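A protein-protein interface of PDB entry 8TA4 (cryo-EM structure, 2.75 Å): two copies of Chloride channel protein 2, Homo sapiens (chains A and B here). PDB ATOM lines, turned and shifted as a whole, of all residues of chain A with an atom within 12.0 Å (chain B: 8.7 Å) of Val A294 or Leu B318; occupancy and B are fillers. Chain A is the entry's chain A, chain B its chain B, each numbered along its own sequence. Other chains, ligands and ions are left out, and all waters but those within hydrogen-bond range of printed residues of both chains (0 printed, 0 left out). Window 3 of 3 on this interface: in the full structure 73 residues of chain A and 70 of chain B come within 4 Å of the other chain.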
ATOM      1  N   TRP A 106      -4.255 -15.676  14.837  1.00  0.00           N
ATOM      2  CA  TRP A 106      -4.400 -14.227  14.760  1.00  0.00           C
ATOM      3  C   TRP A 106      -3.389 -13.520  15.653  1.00  0.00           C
ATOM      4  O   TRP A 106      -2.736 -12.557  15.230  1.00  0.00           O
ATOM      5  CB  TRP A 106      -5.824 -13.816  15.131  1.00  0.00           C
ATOM      6  CG  TRP A 106      -6.074 -12.358  14.940  1.00  0.00           C
ATOM      7  CD1 TRP A 106      -6.511 -11.746  13.807  1.00  0.00           C
ATOM      8  CD2 TRP A 106      -5.885 -11.321  15.909  1.00  0.00           C
ATOM      9  NE1 TRP A 106      -6.609 -10.393  14.008  1.00  0.00           N
ATOM     10  CE2 TRP A 106      -6.230 -10.107  15.292  1.00  0.00           C
ATOM     11  CE3 TRP A 106      -5.457 -11.303  17.238  1.00  0.00           C
ATOM     12  CZ2 TRP A 106      -6.164  -8.888  15.958  1.00  0.00           C
ATOM     13  CZ3 TRP A 106      -5.389 -10.093  17.896  1.00  0.00           C
ATOM     14  CH2 TRP A 106      -5.742  -8.902  17.256  1.00  0.00           C
ATOM     15  N   THR A 283     -13.911 -24.946   8.264  1.00  0.00           N
ATOM     16  CA  THR A 283     -14.967 -23.975   7.998  1.00  0.00           C
ATOM     17  C   THR A 283     -15.199 -23.073   9.201  1.00  0.00           C
ATOM     18  O   THR A 283     -15.380 -21.857   9.050  1.00  0.00           O
ATOM     19  CB  THR A 283     -16.260 -24.694   7.618  1.00  0.00           C
ATOM     20  OG1 THR A 283     -15.983 -25.686   6.625  1.00  0.00           O
ATOM     21  CG2 THR A 283     -17.275 -23.712   7.081  1.00  0.00           C
ATOM     22  N   PHE A 284     -15.205 -23.646  10.406  1.00  0.00           N
ATOM     23  CA  PHE A 284     -15.401 -22.811  11.590  1.00  0.00           C
ATOM     24  C   PHE A 284     -14.248 -21.828  11.780  1.00  0.00           C
ATOM     25  O   PHE A 284     -14.465 -20.666  12.154  1.00  0.00           O
ATOM     26  CB  PHE A 284     -15.585 -23.673  12.835  1.00  0.00           C
ATOM     27  CG  PHE A 284     -16.214 -22.937  13.976  1.00  0.00           C
ATOM     28  CD1 PHE A 284     -17.574 -22.713  14.002  1.00  0.00           C
ATOM     29  CD2 PHE A 284     -15.444 -22.445  15.009  1.00  0.00           C
ATOM     30  CE1 PHE A 284     -18.154 -22.025  15.043  1.00  0.00           C
ATOM     31  CE2 PHE A 284     -16.019 -21.757  16.049  1.00  0.00           C
ATOM     32  CZ  PHE A 284     -17.373 -21.545  16.067  1.00  0.00           C
ATOM     33  N   SER A 285     -13.013 -22.271  11.530  1.00  0.00           N
ATOM     34  CA  SER A 285     -11.874 -21.356  11.612  1.00  0.00           C
ATOM     35  C   SER A 285     -11.995 -20.222  10.604  1.00  0.00           C
ATOM     36  O   SER A 285     -11.687 -19.067  10.917  1.00  0.00           O
ATOM     37  CB  SER A 285     -10.567 -22.112  11.396  1.00  0.00           C
ATOM     38  OG  SER A 285     -10.296 -22.977  12.479  1.00  0.00           O
ATOM     39  N   ALA A 286     -12.430 -20.531   9.381  1.00  0.00           N
ATOM     40  CA  ALA A 286     -12.606 -19.489   8.374  1.00  0.00           C
ATOM     41  C   ALA A 286     -13.677 -18.488   8.791  1.00  0.00           C
ATOM     42  O   ALA A 286     -13.526 -17.277   8.582  1.00  0.00           O
ATOM     43  CB  ALA A 286     -12.955 -20.115   7.028  1.00  0.00           C
ATOM     44  N   PHE A 287     -14.770 -18.974   9.380  1.00  0.00           N
ATOM     45  CA  PHE A 287     -15.806 -18.069   9.869  1.00  0.00           C
ATOM     46  C   PHE A 287     -15.271 -17.143  10.955  1.00  0.00           C
ATOM     47  O   PHE A 287     -15.558 -15.938  10.955  1.00  0.00           O
ATOM     48  CB  PHE A 287     -16.997 -18.872  10.384  1.00  0.00           C
ATOM     49  CG  PHE A 287     -17.947 -18.075  11.230  1.00  0.00           C
ATOM     50  CD1 PHE A 287     -18.763 -17.114  10.663  1.00  0.00           C
ATOM     51  CD2 PHE A 287     -18.028 -18.293  12.592  1.00  0.00           C
ATOM     52  CE1 PHE A 287     -19.632 -16.385  11.440  1.00  0.00           C
ATOM     53  CE2 PHE A 287     -18.896 -17.562  13.371  1.00  0.00           C
ATOM     54  CZ  PHE A 287     -19.700 -16.609  12.795  1.00  0.00           C
ATOM     55  N   ILE A 288     -14.490 -17.686  11.892  1.00  0.00           N
ATOM     56  CA  ILE A 288     -13.922 -16.852  12.950  1.00  0.00           C
ATOM     57  C   ILE A 288     -12.971 -15.813  12.365  1.00  0.00           C
ATOM     58  O   ILE A 288     -12.952 -14.654  12.798  1.00  0.00           O
ATOM     59  CB  ILE A 288     -13.226 -17.722  14.012  1.00  0.00           C
ATOM     60  CG1 ILE A 288     -14.235 -18.645  14.690  1.00  0.00           C
ATOM     61  CG2 ILE A 288     -12.546 -16.852  15.045  1.00  0.00           C
ATOM     62  CD1 ILE A 288     -15.147 -17.939  15.658  1.00  0.00           C
ATOM     63  N   PHE A 289     -12.161 -16.209  11.382  1.00  0.00           N
ATOM     64  CA  PHE A 289     -11.258 -15.251  10.749  1.00  0.00           C
ATOM     65  C   PHE A 289     -12.033 -14.123  10.086  1.00  0.00           C
ATOM     66  O   PHE A 289     -11.645 -12.954  10.186  1.00  0.00           O
ATOM     67  CB  PHE A 289     -10.364 -15.951   9.726  1.00  0.00           C
ATOM     68  CG  PHE A 289      -9.153 -16.603  10.324  1.00  0.00           C
ATOM     69  CD1 PHE A 289      -8.433 -15.974  11.322  1.00  0.00           C
ATOM     70  CD2 PHE A 289      -8.735 -17.846   9.886  1.00  0.00           C
ATOM     71  CE1 PHE A 289      -7.322 -16.574  11.872  1.00  0.00           C
ATOM     72  CE2 PHE A 289      -7.628 -18.447  10.432  1.00  0.00           C
ATOM     73  CZ  PHE A 289      -6.920 -17.810  11.426  1.00  0.00           C
ATOM     74  N   ARG A 290     -13.125 -14.454   9.394  1.00  0.00           N
ATOM     75  CA  ARG A 290     -13.930 -13.423   8.749  1.00  0.00           C
ATOM     76  C   ARG A 290     -14.535 -12.469   9.770  1.00  0.00           C
ATOM     77  O   ARG A 290     -14.545 -11.249   9.565  1.00  0.00           O
ATOM     78  CB  ARG A 290     -15.022 -14.070   7.902  1.00  0.00           C
ATOM     79  CG  ARG A 290     -15.881 -13.083   7.149  1.00  0.00           C
ATOM     80  CD  ARG A 290     -15.064 -12.333   6.126  1.00  0.00           C
ATOM     81  NE  ARG A 290     -15.038 -13.009   4.836  1.00  0.00           N
ATOM     82  CZ  ARG A 290     -15.736 -12.623   3.778  1.00  0.00           C
ATOM     83  NH1 ARG A 290     -16.539 -11.573   3.828  1.00  0.00           N
ATOM     84  NH2 ARG A 290     -15.626 -13.304   2.643  1.00  0.00           N
ATOM     85  N   VAL A 291     -15.043 -13.007  10.881  1.00  0.00           N
ATOM     86  CA  VAL A 291     -15.624 -12.149  11.912  1.00  0.00           C
ATOM     87  C   VAL A 291     -14.569 -11.221  12.498  1.00  0.00           C
ATOM     88  O   VAL A 291     -14.817 -10.027  12.699  1.00  0.00           O
ATOM     89  CB  VAL A 291     -16.302 -12.997  13.000  1.00  0.00           C
ATOM     90  CG1 VAL A 291     -16.533 -12.169  14.246  1.00  0.00           C
ATOM     91  CG2 VAL A 291     -17.610 -13.544  12.484  1.00  0.00           C
ATOM     92  N   LEU A 292     -13.375 -11.748  12.784  1.00  0.00           N
ATOM     93  CA  LEU A 292     -12.312 -10.907  13.330  1.00  0.00           C
ATOM     94  C   LEU A 292     -11.897  -9.825  12.344  1.00  0.00           C
ATOM     95  O   LEU A 292     -11.670  -8.673  12.735  1.00  0.00           O
ATOM     96  CB  LEU A 292     -11.106 -11.761  13.723  1.00  0.00           C
ATOM     97  CG  LEU A 292     -11.190 -12.462  15.079  1.00  0.00           C
ATOM     98  CD1 LEU A 292     -10.062 -13.464  15.243  1.00  0.00           C
ATOM     99  CD2 LEU A 292     -11.167 -11.448  16.198  1.00  0.00           C
ATOM    100  N   ALA A 293     -11.786 -10.173  11.061  1.00  0.00           N
ATOM    101  CA  ALA A 293     -11.407  -9.181  10.061  1.00  0.00           C
ATOM    102  C   ALA A 293     -12.450  -8.078   9.956  1.00  0.00           C
ATOM    103  O   ALA A 293     -12.105  -6.897   9.855  1.00  0.00           O
ATOM    104  CB  ALA A 293     -11.195  -9.850   8.703  1.00  0.00           C
ATOM    105  N   VAL A 294     -13.733  -8.440   9.982  1.00  0.00           N
ATOM    106  CA  VAL A 294     -14.776  -7.417   9.941  1.00  0.00           C
ATOM    107  C   VAL A 294     -14.723  -6.549  11.194  1.00  0.00           C
ATOM    108  O   VAL A 294     -14.901  -5.326  11.128  1.00  0.00           O
ATOM    109  CB  VAL A 294     -16.158  -8.071   9.752  1.00  0.00           C
ATOM    110  CG1 VAL A 294     -17.206  -7.396  10.629  1.00  0.00           C
ATOM    111  CG2 VAL A 294     -16.564  -8.016   8.286  1.00  0.00           C
ATOM    112  N   TRP A 295     -14.465  -7.160  12.351  1.00  0.00           N
ATOM    113  CA  TRP A 295     -14.432  -6.410  13.600  1.00  0.00           C
ATOM    114  C   TRP A 295     -13.230  -5.477  13.694  1.00  0.00           C
ATOM    115  O   TRP A 295     -13.317  -4.447  14.370  1.00  0.00           O
ATOM    116  CB  TRP A 295     -14.458  -7.382  14.784  1.00  0.00           C
ATOM    117  CG  TRP A 295     -13.811  -6.873  16.030  1.00  0.00           C
ATOM    118  CD1 TRP A 295     -12.701  -7.377  16.638  1.00  0.00           C
ATOM    119  CD2 TRP A 295     -14.241  -5.768  16.833  1.00  0.00           C
ATOM    120  NE1 TRP A 295     -12.404  -6.649  17.764  1.00  0.00           N
ATOM    121  CE2 TRP A 295     -13.336  -5.656  17.907  1.00  0.00           C
ATOM    122  CE3 TRP A 295     -15.300  -4.859  16.745  1.00  0.00           C
ATOM    123  CZ2 TRP A 295     -13.457  -4.672  18.885  1.00  0.00           C
ATOM    124  CZ3 TRP A 295     -15.418  -3.883  17.717  1.00  0.00           C
ATOM    125  CH2 TRP A 295     -14.503  -3.797  18.772  1.00  0.00           C
ATOM    126  N   ASN A 296     -12.119  -5.794  13.026  1.00  0.00           N
ATOM    127  CA  ASN A 296     -10.947  -4.923  13.044  1.00  0.00           C
ATOM    128  C   ASN A 296     -10.714  -4.235  11.706  1.00  0.00           C
ATOM    129  O   ASN A 296     -10.812  -3.007  11.625  1.00  0.00           O
ATOM    130  CB  ASN A 296      -9.698  -5.723  13.441  1.00  0.00           C
ATOM    131  CG  ASN A 296      -9.677  -6.084  14.907  1.00  0.00           C
ATOM    132  OD1 ASN A 296     -10.503  -5.612  15.686  1.00  0.00           O
ATOM    133  ND2 ASN A 296      -8.731  -6.929  15.294  1.00  0.00           N
ATOM    134  N   ARG A 297     -10.455  -4.998  10.646  1.00  0.00           N
ATOM    135  CA  ARG A 297     -10.169  -4.448   9.320  1.00  0.00           C
ATOM    136  C   ARG A 297      -9.953  -5.560   8.298  1.00  0.00           C
ATOM    137  O   ARG A 297      -8.866  -5.699   7.737  1.00  0.00           O
ATOM    138  CB  ARG A 297      -8.942  -3.536   9.351  1.00  0.00           C
ATOM    139  CG  ARG A 297      -8.959  -2.469   8.272  1.00  0.00           C
ATOM    140  CD  ARG A 297     -10.301  -1.757   8.219  1.00  0.00           C
ATOM    141  NE  ARG A 297     -10.650  -1.144   9.495  1.00  0.00           N
ATOM    142  CZ  ARG A 297     -10.540   0.150   9.756  1.00  0.00           C
ATOM    143  NH1 ARG A 297     -10.097   1.004   8.846  1.00  0.00           N
ATOM    144  NH2 ARG A 297     -10.886   0.602  10.958  1.00  0.00           N
ATOM    145  N   ALA A 304      -7.905 -13.325   0.211  1.00  0.00           N
ATOM    146  CA  ALA A 304      -7.560 -12.427   1.305  1.00  0.00           C
ATOM    147  C   ALA A 304      -6.102 -11.993   1.236  1.00  0.00           C
ATOM    148  O   ALA A 304      -5.791 -10.813   1.439  1.00  0.00           O
ATOM    149  CB  ALA A 304      -7.859 -13.096   2.646  1.00  0.00           C
ATOM    150  N   PHE B 314     -17.797  -6.805  -2.432  1.00  0.00           N
ATOM    151  CA  PHE B 314     -18.781  -7.120  -1.404  1.00  0.00           C
ATOM    152  C   PHE B 314     -19.948  -7.938  -1.967  1.00  0.00           C
ATOM    153  O   PHE B 314     -21.079  -7.451  -2.031  1.00  0.00           O
ATOM    154  CB  PHE B 314     -19.290  -5.851  -0.734  1.00  0.00           C
ATOM    155  CG  PHE B 314     -18.212  -5.025  -0.094  1.00  0.00           C
ATOM    156  CD1 PHE B 314     -17.777  -5.304   1.189  1.00  0.00           C
ATOM    157  CD2 PHE B 314     -17.639  -3.963  -0.772  1.00  0.00           C
ATOM    158  CE1 PHE B 314     -16.786  -4.542   1.781  1.00  0.00           C
ATOM    159  CE2 PHE B 314     -16.650  -3.200  -0.188  1.00  0.00           C
ATOM    160  CZ  PHE B 314     -16.223  -3.490   1.090  1.00  0.00           C
ATOM    161  N   PRO B 315     -19.698  -9.178  -2.400  1.00  0.00           N
ATOM    162  CA  PRO B 315     -20.800  -9.997  -2.930  1.00  0.00           C
ATOM    163  C   PRO B 315     -21.881 -10.274  -1.907  1.00  0.00           C
ATOM    164  O   PRO B 315     -23.061 -10.356  -2.267  1.00  0.00           O
ATOM    165  CB  PRO B 315     -20.100 -11.292  -3.368  1.00  0.00           C
ATOM    166  CG  PRO B 315     -18.636 -10.991  -3.343  1.00  0.00           C
ATOM    167  CD  PRO B 315     -18.446  -9.943  -2.308  1.00  0.00           C
ATOM    168  N   PHE B 316     -21.511 -10.419  -0.637  1.00  0.00           N
ATOM    169  CA  PHE B 316     -22.460 -10.700   0.428  1.00  0.00           C
ATOM    170  C   PHE B 316     -21.978 -10.012   1.696  1.00  0.00           C
ATOM    171  O   PHE B 316     -20.811  -9.635   1.816  1.00  0.00           O
ATOM    172  CB  PHE B 316     -22.631 -12.210   0.653  1.00  0.00           C
ATOM    173  CG  PHE B 316     -21.397 -12.894   1.171  1.00  0.00           C
ATOM    174  CD1 PHE B 316     -20.400 -13.298   0.308  1.00  0.00           C
ATOM    175  CD2 PHE B 316     -21.240 -13.137   2.522  1.00  0.00           C
ATOM    176  CE1 PHE B 316     -19.270 -13.922   0.782  1.00  0.00           C
ATOM    177  CE2 PHE B 316     -20.110 -13.759   2.999  1.00  0.00           C
ATOM    178  CZ  PHE B 316     -19.127 -14.152   2.129  1.00  0.00           C
ATOM    179  N   ASP B 317     -22.895  -9.847   2.639  1.00  0.00           N
ATOM    180  CA  ASP B 317     -22.600  -9.204   3.908  1.00  0.00           C
ATOM    181  C   ASP B 317     -22.474 -10.239   5.019  1.00  0.00           C
ATOM    182  O   ASP B 317     -22.896 -11.389   4.890  1.00  0.00           O
ATOM    183  CB  ASP B 317     -23.687  -8.182   4.250  1.00  0.00           C
ATOM    184  CG  ASP B 317     -23.216  -7.128   5.229  1.00  0.00           C
ATOM    185  OD1 ASP B 317     -22.369  -6.297   4.845  1.00  0.00           O
ATOM    186  OD2 ASP B 317     -23.693  -7.126   6.381  1.00  0.00           O
ATOM    187  N   LEU B 318     -21.882  -9.807   6.130  1.00  0.00           N
ATOM    188  CA  LEU B 318     -21.714 -10.661   7.297  1.00  0.00           C
ATOM    189  C   LEU B 318     -23.025 -10.945   8.015  1.00  0.00           C
ATOM    190  O   LEU B 318     -23.073 -11.859   8.843  1.00  0.00           O
ATOM    191  CB  LEU B 318     -20.721 -10.017   8.267  1.00  0.00           C
ATOM    192  CG  LEU B 318     -20.026 -10.923   9.283  1.00  0.00           C
ATOM    193  CD1 LEU B 318     -18.832 -11.597   8.644  1.00  0.00           C
ATOM    194  CD2 LEU B 318     -19.604 -10.133  10.502  1.00  0.00           C
ATOM    195  N   GLN B 319     -24.080 -10.190   7.726  1.00  0.00           N
ATOM    196  CA  GLN B 319     -25.387 -10.400   8.328  1.00  0.00           C
ATOM    197  C   GLN B 319     -26.254 -11.372   7.543  1.00  0.00           C
ATOM    198  O   GLN B 319     -27.364 -11.682   7.983  1.00  0.00           O
ATOM    199  CB  GLN B 319     -26.122  -9.065   8.467  1.00  0.00           C
ATOM    200  CG  GLN B 319     -26.026  -8.432   9.840  1.00  0.00           C
ATOM    201  CD  GLN B 319     -26.094  -6.924   9.782  1.00  0.00           C
ATOM    202  OE1 GLN B 319     -25.134  -6.265   9.387  1.00  0.00           O
ATOM    203  NE2 GLN B 319     -27.232  -6.366  10.170  1.00  0.00           N
ATOM    204  N   GLU B 320     -25.784 -11.854   6.395  1.00  0.00           N
ATOM    205  CA  GLU B 320     -26.528 -12.810   5.589  1.00  0.00           C
ATOM    206  C   GLU B 320     -26.128 -14.255   5.846  1.00  0.00           C
ATOM    207  O   GLU B 320     -26.730 -15.157   5.256  1.00  0.00           O
ATOM    208  CB  GLU B 320     -26.350 -12.498   4.101  1.00  0.00           C
ATOM    209  CG  GLU B 320     -27.184 -11.334   3.611  1.00  0.00           C
ATOM    210  CD  GLU B 320     -26.713 -10.805   2.276  1.00  0.00           C
ATOM    211  OE1 GLU B 320     -26.291 -11.614   1.429  1.00  0.00           O
ATOM    212  OE2 GLU B 320     -26.762  -9.578   2.068  1.00  0.00           O
ATOM    213  N   LEU B 321     -25.123 -14.495   6.684  1.00  0.00           N
ATOM    214  CA  LEU B 321     -24.710 -15.864   6.982  1.00  0.00           C
ATOM    215  C   LEU B 321     -25.802 -16.714   7.631  1.00  0.00           C
ATOM    216  O   LEU B 321     -25.871 -17.916   7.315  1.00  0.00           O
ATOM    217  CB  LEU B 321     -23.438 -15.839   7.837  1.00  0.00           C
ATOM    218  CG  LEU B 321     -22.203 -15.276   7.128  1.00  0.00           C
ATOM    219  CD1 LEU B 321     -20.964 -15.412   7.986  1.00  0.00           C
ATOM    220  CD2 LEU B 321     -21.994 -15.954   5.796  1.00  0.00           C
ATOM    221  N   PRO B 322     -26.638 -16.203   8.546  1.00  0.00           N
ATOM    222  CA  PRO B 322     -27.750 -17.031   9.045  1.00  0.00           C
ATOM    223  C   PRO B 322     -28.681 -17.537   7.955  1.00  0.00           C
ATOM    224  O   PRO B 322     -29.234 -18.636   8.089  1.00  0.00           O
ATOM    225  CB  PRO B 322     -28.482 -16.092  10.010  1.00  0.00           C
ATOM    226  CG  PRO B 322     -27.488 -15.106  10.424  1.00  0.00           C
ATOM    227  CD  PRO B 322     -26.477 -14.970   9.337  1.00  0.00           C
ATOM    228  N   ALA B 323     -28.876 -16.772   6.878  1.00  0.00           N
ATOM    229  CA  ALA B 323     -29.676 -17.263   5.760  1.00  0.00           C
ATOM    230  C   ALA B 323     -29.037 -18.488   5.117  1.00  0.00           C
ATOM    231  O   ALA B 323     -29.727 -19.464   4.796  1.00  0.00           O
ATOM    232  CB  ALA B 323     -29.868 -16.153   4.729  1.00  0.00           C
ATOM    233  N   PHE B 324     -27.717 -18.461   4.928  1.00  0.00           N
ATOM    234  CA  PHE B 324     -27.028 -19.615   4.359  1.00  0.00           C
ATOM    235  C   PHE B 324     -27.061 -20.807   5.310  1.00  0.00           C
ATOM    236  O   PHE B 324     -27.166 -21.957   4.869  1.00  0.00           O
ATOM    237  CB  PHE B 324     -25.593 -19.238   4.001  1.00  0.00           C
ATOM    238  CG  PHE B 324     -25.493 -18.100   3.023  1.00  0.00           C
ATOM    239  CD1 PHE B 324     -26.016 -18.215   1.751  1.00  0.00           C
ATOM    240  CD2 PHE B 324     -24.874 -16.917   3.376  1.00  0.00           C
ATOM    241  CE1 PHE B 324     -25.923 -17.173   0.853  1.00  0.00           C
ATOM    242  CE2 PHE B 324     -24.782 -15.872   2.481  1.00  0.00           C
ATOM    243  CZ  PHE B 324     -25.307 -16.002   1.219  1.00  0.00           C
ATOM    244  N   ILE B 485     -28.934  -4.818   3.310  1.00  0.00           N
ATOM    245  CA  ILE B 485     -28.913  -5.316   4.679  1.00  0.00           C
ATOM    246  C   ILE B 485     -28.225  -4.342   5.628  1.00  0.00           C
ATOM    247  O   ILE B 485     -28.464  -4.394   6.841  1.00  0.00           O
ATOM    248  CB  ILE B 485     -28.240  -6.698   4.727  1.00  0.00           C
ATOM    249  CG1 ILE B 485     -28.579  -7.423   6.029  1.00  0.00           C
ATOM    250  CG2 ILE B 485     -26.750  -6.562   4.570  1.00  0.00           C
ATOM    251  CD1 ILE B 485     -29.759  -8.345   5.915  1.00  0.00           C
ATOM    252  N   HIS B 486     -27.384  -3.451   5.111  1.00  0.00           N
ATOM    253  CA  HIS B 486     -26.743  -2.406   5.896  1.00  0.00           C
ATOM    254  C   HIS B 486     -27.090  -1.051   5.299  1.00  0.00           C
ATOM    255  O   HIS B 486     -27.082  -0.882   4.075  1.00  0.00           O
ATOM    256  CB  HIS B 486     -25.225  -2.595   5.938  1.00  0.00           C
ATOM    257  CG  HIS B 486     -24.612  -2.842   4.596  1.00  0.00           C
ATOM    258  ND1 HIS B 486     -24.412  -4.109   4.092  1.00  0.00           N
ATOM    259  CD2 HIS B 486     -24.164  -1.985   3.648  1.00  0.00           C
ATOM    260  CE1 HIS B 486     -23.862  -4.023   2.895  1.00  0.00           C
ATOM    261  NE2 HIS B 486     -23.701  -2.746   2.602  1.00  0.00           N
ATOM    262  N   LEU B 532     -17.161 -19.143   1.364  1.00  0.00           N
ATOM    263  CA  LEU B 532     -17.529 -19.360   2.763  1.00  0.00           C
ATOM    264  C   LEU B 532     -18.994 -19.740   2.953  1.00  0.00           C
ATOM    265  O   LEU B 532     -19.265 -20.701   3.697  1.00  0.00           O
ATOM    266  CB  LEU B 532     -17.160 -18.125   3.593  1.00  0.00           C
ATOM    267  CG  LEU B 532     -17.427 -18.237   5.095  1.00  0.00           C
ATOM    268  CD1 LEU B 532     -16.448 -19.192   5.737  1.00  0.00           C
ATOM    269  CD2 LEU B 532     -17.370 -16.880   5.759  1.00  0.00           C
ATOM    270  N   PRO B 533     -19.979 -19.038   2.370  1.00  0.00           N
ATOM    271  CA  PRO B 533     -21.368 -19.503   2.521  1.00  0.00           C
ATOM    272  C   PRO B 533     -21.608 -20.885   1.946  1.00  0.00           C
ATOM    273  O   PRO B 533     -22.363 -21.673   2.530  1.00  0.00           O
ATOM    274  CB  PRO B 533     -22.172 -18.430   1.777  1.00  0.00           C
ATOM    275  CG  PRO B 533     -21.311 -17.245   1.775  1.00  0.00           C
ATOM    276  CD  PRO B 533     -19.928 -17.763   1.636  1.00  0.00           C
ATOM    277  N   ILE B 536     -20.236 -23.394   4.486  1.00  0.00           N
ATOM    278  CA  ILE B 536     -21.086 -23.470   5.675  1.00  0.00           C
ATOM    279  C   ILE B 536     -22.337 -24.288   5.385  1.00  0.00           C
ATOM    280  O   ILE B 536     -22.694 -25.209   6.137  1.00  0.00           O
ATOM    281  CB  ILE B 536     -21.446 -22.056   6.164  1.00  0.00           C
ATOM    282  CG1 ILE B 536     -20.229 -21.362   6.766  1.00  0.00           C
ATOM    283  CG2 ILE B 536     -22.577 -22.108   7.168  1.00  0.00           C
ATOM    284  CD1 ILE B 536     -20.428 -19.883   6.981  1.00  0.00           C
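Among the printed residues, pairs that only touch across the chains: Thr A283 with Ile B536 (3.8 Å), Ala A286 with Leu B532 (3.8 Å), Phe A287 with Leu B321 (3.8 Å), Arg A290 with Phe B316 (3.6 Å), Arg A290 with Leu B318 (3.6 Å) and Val A294 with Leu B318 (3.6 Å).
Of the printed residues of chain B, Thr A283 touches Ile B536.
Of the printed residues of chain B, Ala A286 touches Leu B532 (3.8 Å).
Of the printed residues of chain B, Phe A287 touches Leu B321 (3.8 Å).
No residue of chain B comes within 4 Å of Ala A293.
Val A294 touches one residue of chain B.
Printed residues of chain A within 4 Å of Phe B316: Arg A290 (3.6 Å).
Leu B318 touches two residues of chain A.
No residue of chain A comes within 4 Å of Gln B319.
No residue of chain A comes within 4 Å of Glu B320.
Of the printed residues of chain A, Leu B532 touches Ala A286 (3.8 Å).
Along chain A the printed residues that touch a printed residue of chain B span positions 283 to 294.
No position is printed for both chains.
Of the 6 pairs that touch across the chains among the printed residues, none has its exchanged pair printed and touching as well.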
